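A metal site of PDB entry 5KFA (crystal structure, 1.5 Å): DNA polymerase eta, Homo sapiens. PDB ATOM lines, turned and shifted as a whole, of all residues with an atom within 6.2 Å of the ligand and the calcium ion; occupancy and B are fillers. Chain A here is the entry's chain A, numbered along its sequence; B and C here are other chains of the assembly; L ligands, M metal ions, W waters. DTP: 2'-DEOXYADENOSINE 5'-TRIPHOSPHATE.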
ATOM      1  N   ASP A  16      -5.702  30.718  18.716  1.00  0.00           N
ATOM      2  CA  ASP A  16      -6.712  30.184  19.614  1.00  0.00           C
ATOM      3  C   ASP A  16      -6.242  30.304  21.082  1.00  0.00           C
ATOM      4  O   ASP A  16      -5.334  29.669  21.477  1.00  0.00           O
ATOM      5  CB  ASP A  16      -6.932  28.734  19.224  1.00  0.00           C
ATOM      6  CG  ASP A  16      -8.131  28.085  19.824  1.00  0.00           C
ATOM      7  OD1 ASP A  16      -8.637  28.588  20.768  1.00  0.00           O
ATOM      8  OD2 ASP A  16      -8.532  27.029  19.293  1.00  0.00           O
ATOM      9  N   MET A  17      -6.960  31.085  21.865  1.00  0.00           N
ATOM     10  CA  MET A  17      -6.549  31.263  23.260  1.00  0.00           C
ATOM     11  C   MET A  17      -6.630  29.941  24.024  1.00  0.00           C
ATOM     12  O   MET A  17      -7.536  29.155  23.803  1.00  0.00           O
ATOM     13  CB  MET A  17      -7.426  32.327  23.947  1.00  0.00           C
ATOM     14  CG  MET A  17      -7.445  33.659  23.201  1.00  0.00           C
ATOM     15  SD  MET A  17      -5.813  34.365  22.866  1.00  0.00           S
ATOM     16  CE  MET A  17      -5.240  34.602  24.519  1.00  0.00           C
ATOM     17  N   ASP A  18      -5.653  29.676  24.892  1.00  0.00           N
ATOM     18  CA  ASP A  18      -5.729  28.440  25.692  1.00  0.00           C
ATOM     19  C   ASP A  18      -6.696  28.584  26.850  1.00  0.00           C
ATOM     20  O   ASP A  18      -6.640  29.583  27.585  1.00  0.00           O
ATOM     21  CB  ASP A  18      -4.369  28.079  26.287  1.00  0.00           C
ATOM     22  CG  ASP A  18      -3.307  27.836  25.223  1.00  0.00           C
ATOM     23  OD1 ASP A  18      -3.646  27.347  24.132  1.00  0.00           O
ATOM     24  OD2 ASP A  18      -2.148  28.126  25.501  1.00  0.00           O
ATOM     25  N   CYS A  19      -7.563  27.578  26.986  1.00  0.00           N
ATOM     26  CA  CYS A  19      -8.578  27.507  28.064  1.00  0.00           C
ATOM     27  C   CYS A  19      -9.046  28.903  28.473  1.00  0.00           C
ATOM     28  O   CYS A  19      -8.851  29.336  29.618  1.00  0.00           O
ATOM     29  CB  CYS A  19      -8.081  26.699  29.273  1.00  0.00           C
ATOM     30  SG  CYS A  19      -6.534  27.171  30.047  1.00  0.00           S
ATOM     31  N   PHE A  20      -9.651  29.605  27.521  1.00  0.00           N
ATOM     32  CA  PHE A  20      -9.740  31.051  27.594  1.00  0.00           C
ATOM     33  C   PHE A  20     -10.452  31.593  28.836  1.00  0.00           C
ATOM     34  O   PHE A  20      -9.893  32.429  29.544  1.00  0.00           O
ATOM     35  CB  PHE A  20     -10.422  31.602  26.339  1.00  0.00           C
ATOM     36  CG  PHE A  20     -10.453  33.107  26.291  1.00  0.00           C
ATOM     37  CD1 PHE A  20      -9.300  33.841  26.535  1.00  0.00           C
ATOM     38  CD2 PHE A  20     -11.628  33.780  26.005  1.00  0.00           C
ATOM     39  CE1 PHE A  20      -9.322  35.238  26.497  1.00  0.00           C
ATOM     40  CE2 PHE A  20     -11.661  35.185  25.963  1.00  0.00           C
ATOM     41  CZ  PHE A  20     -10.508  35.906  26.202  1.00  0.00           C
ATOM     42  N   PHE A  21     -11.652  31.109  29.140  1.00  0.00           N
ATOM     43  CA  PHE A  21     -12.345  31.709  30.273  1.00  0.00           C
ATOM     44  C   PHE A  21     -11.582  31.430  31.579  1.00  0.00           C
ATOM     45  O   PHE A  21     -11.621  32.243  32.501  1.00  0.00           O
ATOM     46  CB  PHE A  21     -13.783  31.192  30.430  1.00  0.00           C
ATOM     47  CG  PHE A  21     -14.738  31.682  29.380  1.00  0.00           C
ATOM     48  CD1 PHE A  21     -14.313  32.276  28.193  1.00  0.00           C
ATOM     49  CD2 PHE A  21     -16.101  31.539  29.591  1.00  0.00           C
ATOM     50  CE1 PHE A  21     -15.239  32.718  27.245  1.00  0.00           C
ATOM     51  CE2 PHE A  21     -17.035  31.972  28.648  1.00  0.00           C
ATOM     52  CZ  PHE A  21     -16.590  32.563  27.474  1.00  0.00           C
ATOM     53  N   VAL A  22     -10.923  30.276  31.671  1.00  0.00           N
ATOM     54  CA  VAL A  22     -10.095  29.960  32.826  1.00  0.00           C
ATOM     55  C   VAL A  22      -8.962  30.966  32.943  1.00  0.00           C
ATOM     56  O   VAL A  22      -8.695  31.472  34.038  1.00  0.00           O
ATOM     57  CB  VAL A  22      -9.546  28.532  32.735  1.00  0.00           C
ATOM     58  CG1 VAL A  22      -8.376  28.315  33.698  1.00  0.00           C
ATOM     59  CG2 VAL A  22     -10.667  27.529  32.998  1.00  0.00           C
ATOM     60  N   GLN A  41     -21.115  27.775  35.221  1.00  0.00           N
ATOM     61  CA  GLN A  41     -22.225  28.723  35.220  1.00  0.00           C
ATOM     62  C   GLN A  41     -23.346  28.158  36.057  1.00  0.00           C
ATOM     63  O   GLN A  41     -23.659  26.962  35.965  1.00  0.00           O
ATOM     64  CB  GLN A  41     -22.698  29.056  33.802  1.00  0.00           C
ATOM     65  CG  GLN A  41     -22.930  27.877  32.903  1.00  0.00           C
ATOM     66  CD  GLN A  41     -23.098  28.283  31.454  1.00  0.00           C
ATOM     67  OE1 GLN A  41     -22.870  29.439  31.085  1.00  0.00           O
ATOM     68  NE2 GLN A  41     -23.515  27.331  30.622  1.00  0.00           N
ATOM     69  N   ILE A  51     -17.908  25.125  31.749  1.00  0.00           N
ATOM     70  CA  ILE A  51     -17.755  25.593  30.374  1.00  0.00           C
ATOM     71  C   ILE A  51     -16.300  25.809  29.955  1.00  0.00           C
ATOM     72  O   ILE A  51     -16.054  25.990  28.769  1.00  0.00           O
ATOM     73  CB  ILE A  51     -18.556  26.883  30.114  1.00  0.00           C
ATOM     74  CG1 ILE A  51     -18.119  28.030  31.037  1.00  0.00           C
ATOM     75  CG2 ILE A  51     -20.064  26.607  30.250  1.00  0.00           C
ATOM     76  CD1 ILE A  51     -18.760  29.386  30.673  1.00  0.00           C
ATOM     77  N   ALA A  52     -15.357  25.767  30.890  1.00  0.00           N
ATOM     78  CA  ALA A  52     -13.928  25.861  30.545  1.00  0.00           C
ATOM     79  C   ALA A  52     -13.097  25.168  31.599  1.00  0.00           C
ATOM     80  O   ALA A  52     -13.480  25.179  32.769  1.00  0.00           O
ATOM     81  CB  ALA A  52     -13.490  27.326  30.385  1.00  0.00           C
ATOM     82  N   VAL A  53     -11.967  24.561  31.202  1.00  0.00           N
ATOM     83  CA  VAL A  53     -11.182  23.676  32.064  1.00  0.00           C
ATOM     84  C   VAL A  53      -9.684  23.901  31.875  1.00  0.00           C
ATOM     85  O   VAL A  53      -9.195  23.854  30.745  1.00  0.00           O
ATOM     86  CB  VAL A  53     -11.484  22.174  31.769  1.00  0.00           C
ATOM     87  CG1 VAL A  53     -10.809  21.286  32.803  1.00  0.00           C
ATOM     88  CG2 VAL A  53     -12.980  21.899  31.747  1.00  0.00           C
ATOM     89  N   TYR A  55      -5.648  23.099  31.936  1.00  0.00           N
ATOM     90  CA  TYR A  55      -4.966  21.891  31.494  1.00  0.00           C
ATOM     91  C   TYR A  55      -4.594  21.001  32.681  1.00  0.00           C
ATOM     92  O   TYR A  55      -4.615  19.774  32.554  1.00  0.00           O
ATOM     93  CB  TYR A  55      -3.749  22.253  30.635  1.00  0.00           C
ATOM     94  CG  TYR A  55      -4.203  22.605  29.229  1.00  0.00           C
ATOM     95  CD1 TYR A  55      -4.732  23.868  28.945  1.00  0.00           C
ATOM     96  CD2 TYR A  55      -4.198  21.650  28.212  1.00  0.00           C
ATOM     97  CE1 TYR A  55      -5.193  24.175  27.674  1.00  0.00           C
ATOM     98  CE2 TYR A  55      -4.649  21.950  26.945  1.00  0.00           C
ATOM     99  CZ  TYR A  55      -5.156  23.201  26.677  1.00  0.00           C
ATOM    100  OH  TYR A  55      -5.606  23.482  25.398  1.00  0.00           O
ATOM    101  N   ARG A  58      -7.725  19.060  33.215  1.00  0.00           N
ATOM    102  CA  ARG A  58      -7.972  18.076  32.149  1.00  0.00           C
ATOM    103  C   ARG A  58      -7.210  16.764  32.398  1.00  0.00           C
ATOM    104  O   ARG A  58      -7.673  15.694  31.987  1.00  0.00           O
ATOM    105  CB  ARG A  58      -7.595  18.629  30.783  1.00  0.00           C
ATOM    106  CG  ARG A  58      -8.378  19.857  30.397  1.00  0.00           C
ATOM    107  CD  ARG A  58      -7.958  20.387  29.041  1.00  0.00           C
ATOM    108  NE  ARG A  58      -8.457  21.747  28.874  1.00  0.00           N
ATOM    109  CZ  ARG A  58      -8.557  22.389  27.719  1.00  0.00           C
ATOM    110  NH1 ARG A  58      -8.177  21.813  26.590  1.00  0.00           N
ATOM    111  NH2 ARG A  58      -9.038  23.638  27.709  1.00  0.00           N
ATOM    112  N   ARG A  64     -15.553  20.012  29.582  1.00  0.00           N
ATOM    113  CA  ARG A  64     -16.720  20.852  29.334  1.00  0.00           C
ATOM    114  C   ARG A  64     -17.997  19.993  29.359  1.00  0.00           C
ATOM    115  O   ARG A  64     -17.944  18.811  29.017  1.00  0.00           O
ATOM    116  CB  ARG A  64     -16.546  21.591  28.000  1.00  0.00           C
ATOM    117  CG  ARG A  64     -17.762  22.345  27.483  1.00  0.00           C
ATOM    118  CD  ARG A  64     -17.388  23.177  26.266  1.00  0.00           C
ATOM    119  NE  ARG A  64     -16.317  24.116  26.598  1.00  0.00           N
ATOM    120  CZ  ARG A  64     -15.195  24.264  25.894  1.00  0.00           C
ATOM    121  NH1 ARG A  64     -14.995  23.562  24.777  1.00  0.00           N
ATOM    122  NH2 ARG A  64     -14.276  25.142  26.293  1.00  0.00           N
ATOM    123  N   SER A 116     -14.480  33.450  16.688  1.00  0.00           N
ATOM    124  CA  SER A 116     -15.227  33.141  17.904  1.00  0.00           C
ATOM    125  C   SER A 116     -14.764  34.080  18.988  1.00  0.00           C
ATOM    126  O   SER A 116     -13.932  34.938  18.747  1.00  0.00           O
ATOM    127  CB  SER A 116     -15.017  31.697  18.343  1.00  0.00           C
ATOM    128  OG  SER A 116     -13.715  31.533  18.895  1.00  0.00           O
ATOM    129  N   ILE A 117     -15.247  33.872  20.215  1.00  0.00           N
ATOM    130  CA  ILE A 117     -14.847  34.734  21.317  1.00  0.00           C
ATOM    131  C   ILE A 117     -13.330  34.671  21.577  1.00  0.00           C
ATOM    132  O   ILE A 117     -12.757  35.602  22.135  1.00  0.00           O
ATOM    133  CB  ILE A 117     -15.637  34.376  22.603  1.00  0.00           C
ATOM    134  CG1 ILE A 117     -15.534  35.506  23.631  1.00  0.00           C
ATOM    135  CG2 ILE A 117     -15.167  33.043  23.161  1.00  0.00           C
ATOM    136  CD1 ILE A 117     -16.609  35.430  24.712  1.00  0.00           C
ATOM    137  N   ASP A 118     -12.656  33.592  21.171  1.00  0.00           N
ATOM    138  CA  ASP A 118     -11.233  33.504  21.491  1.00  0.00           C
ATOM    139  C   ASP A 118     -10.366  32.980  20.338  1.00  0.00           C
ATOM    140  O   ASP A 118      -9.241  32.518  20.562  1.00  0.00           O
ATOM    141  CB  ASP A 118     -11.040  32.632  22.728  1.00  0.00           C
ATOM    142  CG  ASP A 118     -11.063  31.148  22.407  1.00  0.00           C
ATOM    143  OD1 ASP A 118     -10.312  30.403  23.064  1.00  0.00           O
ATOM    144  OD2 ASP A 118     -11.790  30.737  21.463  1.00  0.00           O
ATOM    145  N   GLU A 119     -10.859  33.084  19.116  1.00  0.00           N
ATOM    146  CA  GLU A 119     -10.150  32.614  17.927  1.00  0.00           C
ATOM    147  C   GLU A 119     -10.186  33.666  16.853  1.00  0.00           C
ATOM    148  O   GLU A 119     -11.170  34.246  16.633  1.00  0.00           O
ATOM    149  CB  GLU A 119     -10.800  31.362  17.331  1.00  0.00           C
ATOM    150  CG  GLU A 119     -10.759  30.113  18.214  1.00  0.00           C
ATOM    151  CD  GLU A 119     -11.224  28.876  17.540  1.00  0.00           C
ATOM    152  OE1 GLU A 119     -11.549  28.935  16.394  1.00  0.00           O
ATOM    153  OE2 GLU A 119     -11.166  27.842  18.155  1.00  0.00           O
ATOM    154  N   LYS A 227      -6.333  26.005  11.184  1.00  0.00           N
ATOM    155  CA  LYS A 227      -7.133  25.548  12.320  1.00  0.00           C
ATOM    156  C   LYS A 227      -6.694  24.149  12.777  1.00  0.00           C
ATOM    157  O   LYS A 227      -6.503  23.909  13.973  1.00  0.00           O
ATOM    158  CB  LYS A 227      -8.621  25.545  11.969  1.00  0.00           C
ATOM    159  CG  LYS A 227      -9.516  24.972  13.053  1.00  0.00           C
ATOM    160  CD  LYS A 227      -9.388  25.737  14.355  1.00  0.00           C
ATOM    161  CE  LYS A 227     -10.337  25.191  15.415  1.00  0.00           C
ATOM    162  NZ  LYS A 227     -10.065  25.801  16.738  1.00  0.00           N
ATOM    163  N   LYS A 234      -1.079  21.851  21.651  1.00  0.00           N
ATOM    164  CA  LYS A 234      -1.673  22.755  22.650  1.00  0.00           C
ATOM    165  C   LYS A 234      -1.211  22.254  24.007  1.00  0.00           C
ATOM    166  O   LYS A 234      -0.975  21.049  24.179  1.00  0.00           O
ATOM    167  CB  LYS A 234      -3.207  22.767  22.561  1.00  0.00           C
ATOM    168  CG  LYS A 234      -3.848  23.866  21.688  1.00  0.00           C
ATOM    169  CD  LYS A 234      -5.331  24.118  22.105  1.00  0.00           C
ATOM    170  CE  LYS A 234      -5.960  25.402  21.508  1.00  0.00           C
ATOM    171  NZ  LYS A 234      -5.770  26.677  22.337  1.00  0.00           N
ATOM    172  N   PRO A 235      -1.063  23.150  24.985  1.00  0.00           N
ATOM    173  CA  PRO A 235      -1.262  24.596  24.903  1.00  0.00           C
ATOM    174  C   PRO A 235       0.055  25.327  24.706  1.00  0.00           C
ATOM    175  O   PRO A 235       1.130  24.713  24.729  1.00  0.00           O
ATOM    176  CB  PRO A 235      -1.850  24.932  26.269  1.00  0.00           C
ATOM    177  CG  PRO A 235      -1.097  23.982  27.188  1.00  0.00           C
ATOM    178  CD  PRO A 235      -0.855  22.714  26.370  1.00  0.00           C
ATOM    179  P    DT B   3     -28.568  17.071  30.561  1.00  0.00           P
ATOM    180  OP1  DT B   3     -29.542  16.018  30.184  1.00  0.00           O
ATOM    181  OP2  DT B   3     -27.258  16.706  31.136  1.00  0.00           O
ATOM    182  O5'  DT B   3     -28.324  17.972  29.266  1.00  0.00           O
ATOM    183  C5'  DT B   3     -27.136  18.739  29.144  1.00  0.00           C
ATOM    184  C4'  DT B   3     -27.214  19.997  29.997  1.00  0.00           C
ATOM    185  O4'  DT B   3     -25.880  20.534  30.169  1.00  0.00           O
ATOM    186  C3'  DT B   3     -28.042  21.122  29.395  1.00  0.00           C
ATOM    187  O3'  DT B   3     -28.613  21.885  30.444  1.00  0.00           O
ATOM    188  C2'  DT B   3     -27.005  21.919  28.633  1.00  0.00           C
ATOM    189  C1'  DT B   3     -25.796  21.812  29.561  1.00  0.00           C
ATOM    190  N1   DT B   3     -24.489  21.913  28.856  1.00  0.00           N
ATOM    191  C2   DT B   3     -23.537  22.797  29.307  1.00  0.00           C
ATOM    192  O2   DT B   3     -23.697  23.520  30.278  1.00  0.00           O
ATOM    193  N3   DT B   3     -22.364  22.797  28.588  1.00  0.00           N
ATOM    194  C4   DT B   3     -22.068  22.018  27.476  1.00  0.00           C
ATOM    195  O4   DT B   3     -20.992  22.082  26.905  1.00  0.00           O
ATOM    196  C5   DT B   3     -23.116  21.107  27.062  1.00  0.00           C
ATOM    197  C7   DT B   3     -22.915  20.212  25.875  1.00  0.00           C
ATOM    198  C6   DT B   3     -24.259  21.092  27.766  1.00  0.00           C
ATOM    199  P    DT B   4     -29.480  23.201  30.116  1.00  0.00           P
ATOM    200  OP1  DT B   4     -30.248  23.540  31.327  1.00  0.00           O
ATOM    201  OP2  DT B   4     -30.173  22.988  28.823  1.00  0.00           O
ATOM    202  O5'  DT B   4     -28.377  24.328  29.879  1.00  0.00           O
ATOM    203  C5'  DT B   4     -27.670  24.842  30.962  1.00  0.00           C
ATOM    204  C4'  DT B   4     -27.012  26.153  30.584  1.00  0.00           C
ATOM    205  O4'  DT B   4     -25.854  25.891  29.774  1.00  0.00           O
ATOM    206  C3'  DT B   4     -27.889  27.103  29.780  1.00  0.00           C
ATOM    207  O3'  DT B   4     -27.612  28.405  30.245  1.00  0.00           O
ATOM    208  C2'  DT B   4     -27.396  26.902  28.346  1.00  0.00           C
ATOM    209  C1'  DT B   4     -25.916  26.671  28.593  1.00  0.00           C
ATOM    210  N1   DT B   4     -25.196  25.924  27.544  1.00  0.00           N
ATOM    211  C2   DT B   4     -23.915  26.307  27.291  1.00  0.00           C
ATOM    212  O2   DT B   4     -23.383  27.249  27.855  1.00  0.00           O
ATOM    213  N3   DT B   4     -23.268  25.556  26.359  1.00  0.00           N
ATOM    214  C4   DT B   4     -23.748  24.488  25.666  1.00  0.00           C
ATOM    215  O4   DT B   4     -23.066  23.883  24.839  1.00  0.00           O
ATOM    216  C5   DT B   4     -25.115  24.107  25.988  1.00  0.00           C
ATOM    217  C7   DT B   4     -25.768  22.940  25.293  1.00  0.00           C
ATOM    218  C6   DT B   4     -25.760  24.836  26.920  1.00  0.00           C
ATOM    219  P    DA B   5     -28.362  29.689  29.651  1.00  0.00           P
ATOM    220  OP1  DA B   5     -28.634  30.565  30.792  1.00  0.00           O
ATOM    221  OP2  DA B   5     -29.475  29.261  28.779  1.00  0.00           O
ATOM    222  O5'  DA B   5     -27.253  30.365  28.746  1.00  0.00           O
ATOM    223  C5'  DA B   5     -26.109  30.956  29.331  1.00  0.00           C
ATOM    224  C4'  DA B   5     -25.248  31.589  28.262  1.00  0.00           C
ATOM    225  O4'  DA B   5     -24.633  30.553  27.442  1.00  0.00           O
ATOM    226  C3'  DA B   5     -26.001  32.504  27.295  1.00  0.00           C
ATOM    227  O3'  DA B   5     -25.195  33.647  27.000  1.00  0.00           O
ATOM    228  C2'  DA B   5     -26.186  31.622  26.064  1.00  0.00           C
ATOM    229  C1'  DA B   5     -24.860  30.870  26.073  1.00  0.00           C
ATOM    230  N9   DA B   5     -24.860  29.647  25.305  1.00  0.00           N
ATOM    231  C8   DA B   5     -25.884  28.762  25.158  1.00  0.00           C
ATOM    232  N7   DA B   5     -25.576  27.724  24.401  1.00  0.00           N
ATOM    233  C5   DA B   5     -24.258  27.948  24.048  1.00  0.00           C
ATOM    234  C6   DA B   5     -23.343  27.219  23.257  1.00  0.00           C
ATOM    235  N6   DA B   5     -23.649  26.066  22.671  1.00  0.00           N
ATOM    236  N1   DA B   5     -22.106  27.729  23.108  1.00  0.00           N
ATOM    237  C2   DA B   5     -21.800  28.886  23.702  1.00  0.00           C
ATOM    238  N3   DA B   5     -22.569  29.654  24.470  1.00  0.00           N
ATOM    239  C4   DA B   5     -23.795  29.122  24.597  1.00  0.00           C
ATOM    240  P    DT C   8     -14.901  24.340  17.453  1.00  0.00           P
ATOM    241  OP1  DT C   8     -13.451  24.230  17.189  1.00  0.00           O
ATOM    242  OP2  DT C   8     -15.554  23.274  18.245  1.00  0.00           O
ATOM    243  O5'  DT C   8     -15.272  25.754  18.166  1.00  0.00           O
ATOM    244  C5'  DT C   8     -14.425  26.893  18.029  1.00  0.00           C
ATOM    245  C4'  DT C   8     -14.912  28.083  18.858  1.00  0.00           C
ATOM    246  O4'  DT C   8     -16.360  28.063  18.975  1.00  0.00           O
ATOM    247  C3'  DT C   8     -14.353  28.187  20.276  1.00  0.00           C
ATOM    248  O3'  DT C   8     -14.021  29.533  20.549  1.00  0.00           O
ATOM    249  C2'  DT C   8     -15.519  27.713  21.146  1.00  0.00           C
ATOM    250  C1'  DT C   8     -16.738  28.151  20.341  1.00  0.00           C
ATOM    251  N1   DT C   8     -17.952  27.293  20.577  1.00  0.00           N
ATOM    252  C2   DT C   8     -18.968  27.777  21.372  1.00  0.00           C
ATOM    253  O2   DT C   8     -18.921  28.869  21.915  1.00  0.00           O
ATOM    254  N3   DT C   8     -20.027  26.927  21.523  1.00  0.00           N
ATOM    255  C4   DT C   8     -20.171  25.666  20.978  1.00  0.00           C
ATOM    256  O4   DT C   8     -21.171  24.973  21.160  1.00  0.00           O
ATOM    257  C5   DT C   8     -19.080  25.219  20.151  1.00  0.00           C
ATOM    258  C7   DT C   8     -19.133  23.871  19.504  1.00  0.00           C
ATOM    259  C6   DT C   8     -18.029  26.046  20.001  1.00  0.00           C
HETATM  260  PG  DTP L   1      -8.646  25.171  24.518  1.00  0.00           P
HETATM  261  O1G DTP L   1      -8.858  26.033  23.286  1.00  0.00           O
HETATM  262  O2G DTP L   1      -7.325  25.476  25.167  1.00  0.00           O
HETATM  263  O3G DTP L   1      -8.808  23.690  24.232  1.00  0.00           O
HETATM  264  PB  DTP L   1     -10.901  26.617  25.521  1.00  0.00           P
HETATM  265  O1B DTP L   1     -10.320  27.944  25.058  1.00  0.00           O
HETATM  266  O2B DTP L   1     -11.574  26.740  26.863  1.00  0.00           O
HETATM  267  O3B DTP L   1      -9.762  25.496  25.620  1.00  0.00           O
HETATM  268  PA  DTP L   1     -12.626  26.730  23.207  1.00  0.00           P
HETATM  269  O1A DTP L   1     -11.581  27.325  22.311  1.00  0.00           O
HETATM  270  O2A DTP L   1     -13.443  25.644  22.552  1.00  0.00           O
HETATM  271  O3A DTP L   1     -11.973  26.043  24.487  1.00  0.00           O
HETATM  272  O5' DTP L   1     -13.635  27.819  23.727  1.00  0.00           O
HETATM  273  C5' DTP L   1     -13.242  29.117  24.113  1.00  0.00           C
HETATM  274  C4' DTP L   1     -14.138  29.603  25.241  1.00  0.00           C
HETATM  275  O4' DTP L   1     -15.466  29.639  24.755  1.00  0.00           O
HETATM  276  C3' DTP L   1     -14.139  28.688  26.370  1.00  0.00           C
HETATM  277  O3' DTP L   1     -13.115  29.033  27.318  1.00  0.00           O
HETATM  278  C2' DTP L   1     -15.470  28.809  26.962  1.00  0.00           C
HETATM  279  C1' DTP L   1     -16.329  29.131  25.782  1.00  0.00           C
HETATM  280  N9  DTP L   1     -17.022  27.984  25.292  1.00  0.00           N
HETATM  281  C8  DTP L   1     -16.567  27.043  24.426  1.00  0.00           C
HETATM  282  N7  DTP L   1     -17.503  26.129  24.203  1.00  0.00           N
HETATM  283  C5  DTP L   1     -18.601  26.449  24.915  1.00  0.00           C
HETATM  284  C6  DTP L   1     -19.863  25.896  25.097  1.00  0.00           C
HETATM  285  N6  DTP L   1     -20.231  24.689  24.418  1.00  0.00           N
HETATM  286  N1  DTP L   1     -20.725  26.491  25.922  1.00  0.00           N
HETATM  287  C2  DTP L   1     -20.434  27.634  26.580  1.00  0.00           C
HETATM  288  N3  DTP L   1     -19.203  28.206  26.422  1.00  0.00           N
HETATM  289  C4  DTP L   1     -18.301  27.637  25.617  1.00  0.00           C
HETATM  290 CA    CA M   1      -9.444  28.228  22.943  1.00  0.00          CA
HETATM  291  O   HOH W   1     -19.756  30.826  27.018  1.00  0.00           O
HETATM  292  O   HOH W   2      -9.465  23.397  21.419  1.00  0.00           O
HETATM  293  O   HOH W   3     -11.726  24.496  28.424  1.00  0.00           O
HETATM  294  O   HOH W   4     -11.047  22.222  24.507  1.00  0.00           O
HETATM  295  O   HOH W   5     -10.708  25.672  20.263  1.00  0.00           O
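OH of Tyr 55 lies within hydrogen-bond range of O2G of the ligand (2.6 Å).
O4 of DT 4 of chain B lies within hydrogen-bond range of N6 of the ligand.
An oxygen (O2G) of the ligand lies within hydrogen-bond range of the backbone NH (N) of Cys 19 (2.8 Å).
The guanidinium group of Arg 58 is in salt-bridge range of an oxygen (O3G) of the ligand, at 3.1 Å.
N of Phe 20 lies close to O1B of the ligand (3.0 Å).
An oxygen (O2B) of the ligand lies within salt-bridge range of the guanidinium group of Arg 64 (3.2 Å).
O3' of the ligand lies within hydrogen-bond range of N of Phe 21 (3.1 Å).
O4 of DT 8 of chain C lies within hydrogen-bond range of N6 of the ligand (3.4 Å).
The side-chain amino group of Lys 234 lies within salt-bridge range of an oxygen (O2G) of the ligand, 3.4 Å away.
The side-chain carboxylate (OD2) of Asp 118 lies close to O3' of DT 8 of chain C (2.7 Å).
The side-chain hydroxyl (OG) of Ser 116 sits close to the backbone NH (N) of Asp 118 (3.2 Å).
The side-chain carboxylate (OD2) of Asp 16 lies within salt-bridge range of the side-chain amino group (NZ) of Lys 227 (3.2 Å).
OH of Tyr 55 lies within hydrogen-bond range of NH1 of Arg 58 (3.3 Å).
NE of Arg 58 sits at hydrogen-bond distance from O of Val 53, at 2.9 Å.
OG of Ser 116 lies within hydrogen-bond range of O3' of DT 8 of chain C (2.6 Å).
OP1 of DT 8 of chain C lies within salt-bridge range of the side-chain amino group (NZ) of Lys 227 (3.8 Å).
The side-chain carboxylate of Asp 18 lies within salt-bridge range of the side-chain amino group of Lys 234 (2.9 Å).
A nitrogen (N1) of the ligand sits close to N1 of DA 5 of chain B (3.4 Å).
CA of Asp 18 touches O2G of the ligand, at 3.4 Å.
O of Ile 51 touches C2' of the ligand (3.4 Å).
CB of Ala 52 touches O3' of the ligand, 3.5 Å away.
Ile 117 touches the ligand (CG2 to O4', 3.8 Å).
DT 3 of chain B touches the ligand.
Hydrophobic or aromatic side chains that line the ligand: Phe 20, Phe 21, Ile 51, Ala 52, Tyr 55 and Ile 117.
Of the 25 residues printed, 18 come within 4 Å of the ligand.
The nearest printed residue that does not touch the ligand is Glu 119 (4.2 Å).
The calcium ion is bound by the backbone carbonyl oxygen of Met 17 (2.3 Å), an oxygen (O1G) of the ligand (2.3 Å), an oxygen (O1B) of the ligand (2.3 Å), the side-chain carboxylate of Asp 118 (2.3 Å), the side-chain carboxylate of Asp 16 (2.3 Å) and an oxygen (O1A) of the ligand (2.4 Å).
Water W5 bridges the side-chain carboxylate of Asp 16 (2.7 Å) and the side-chain carboxylate of Glu 119 (3.1 Å).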
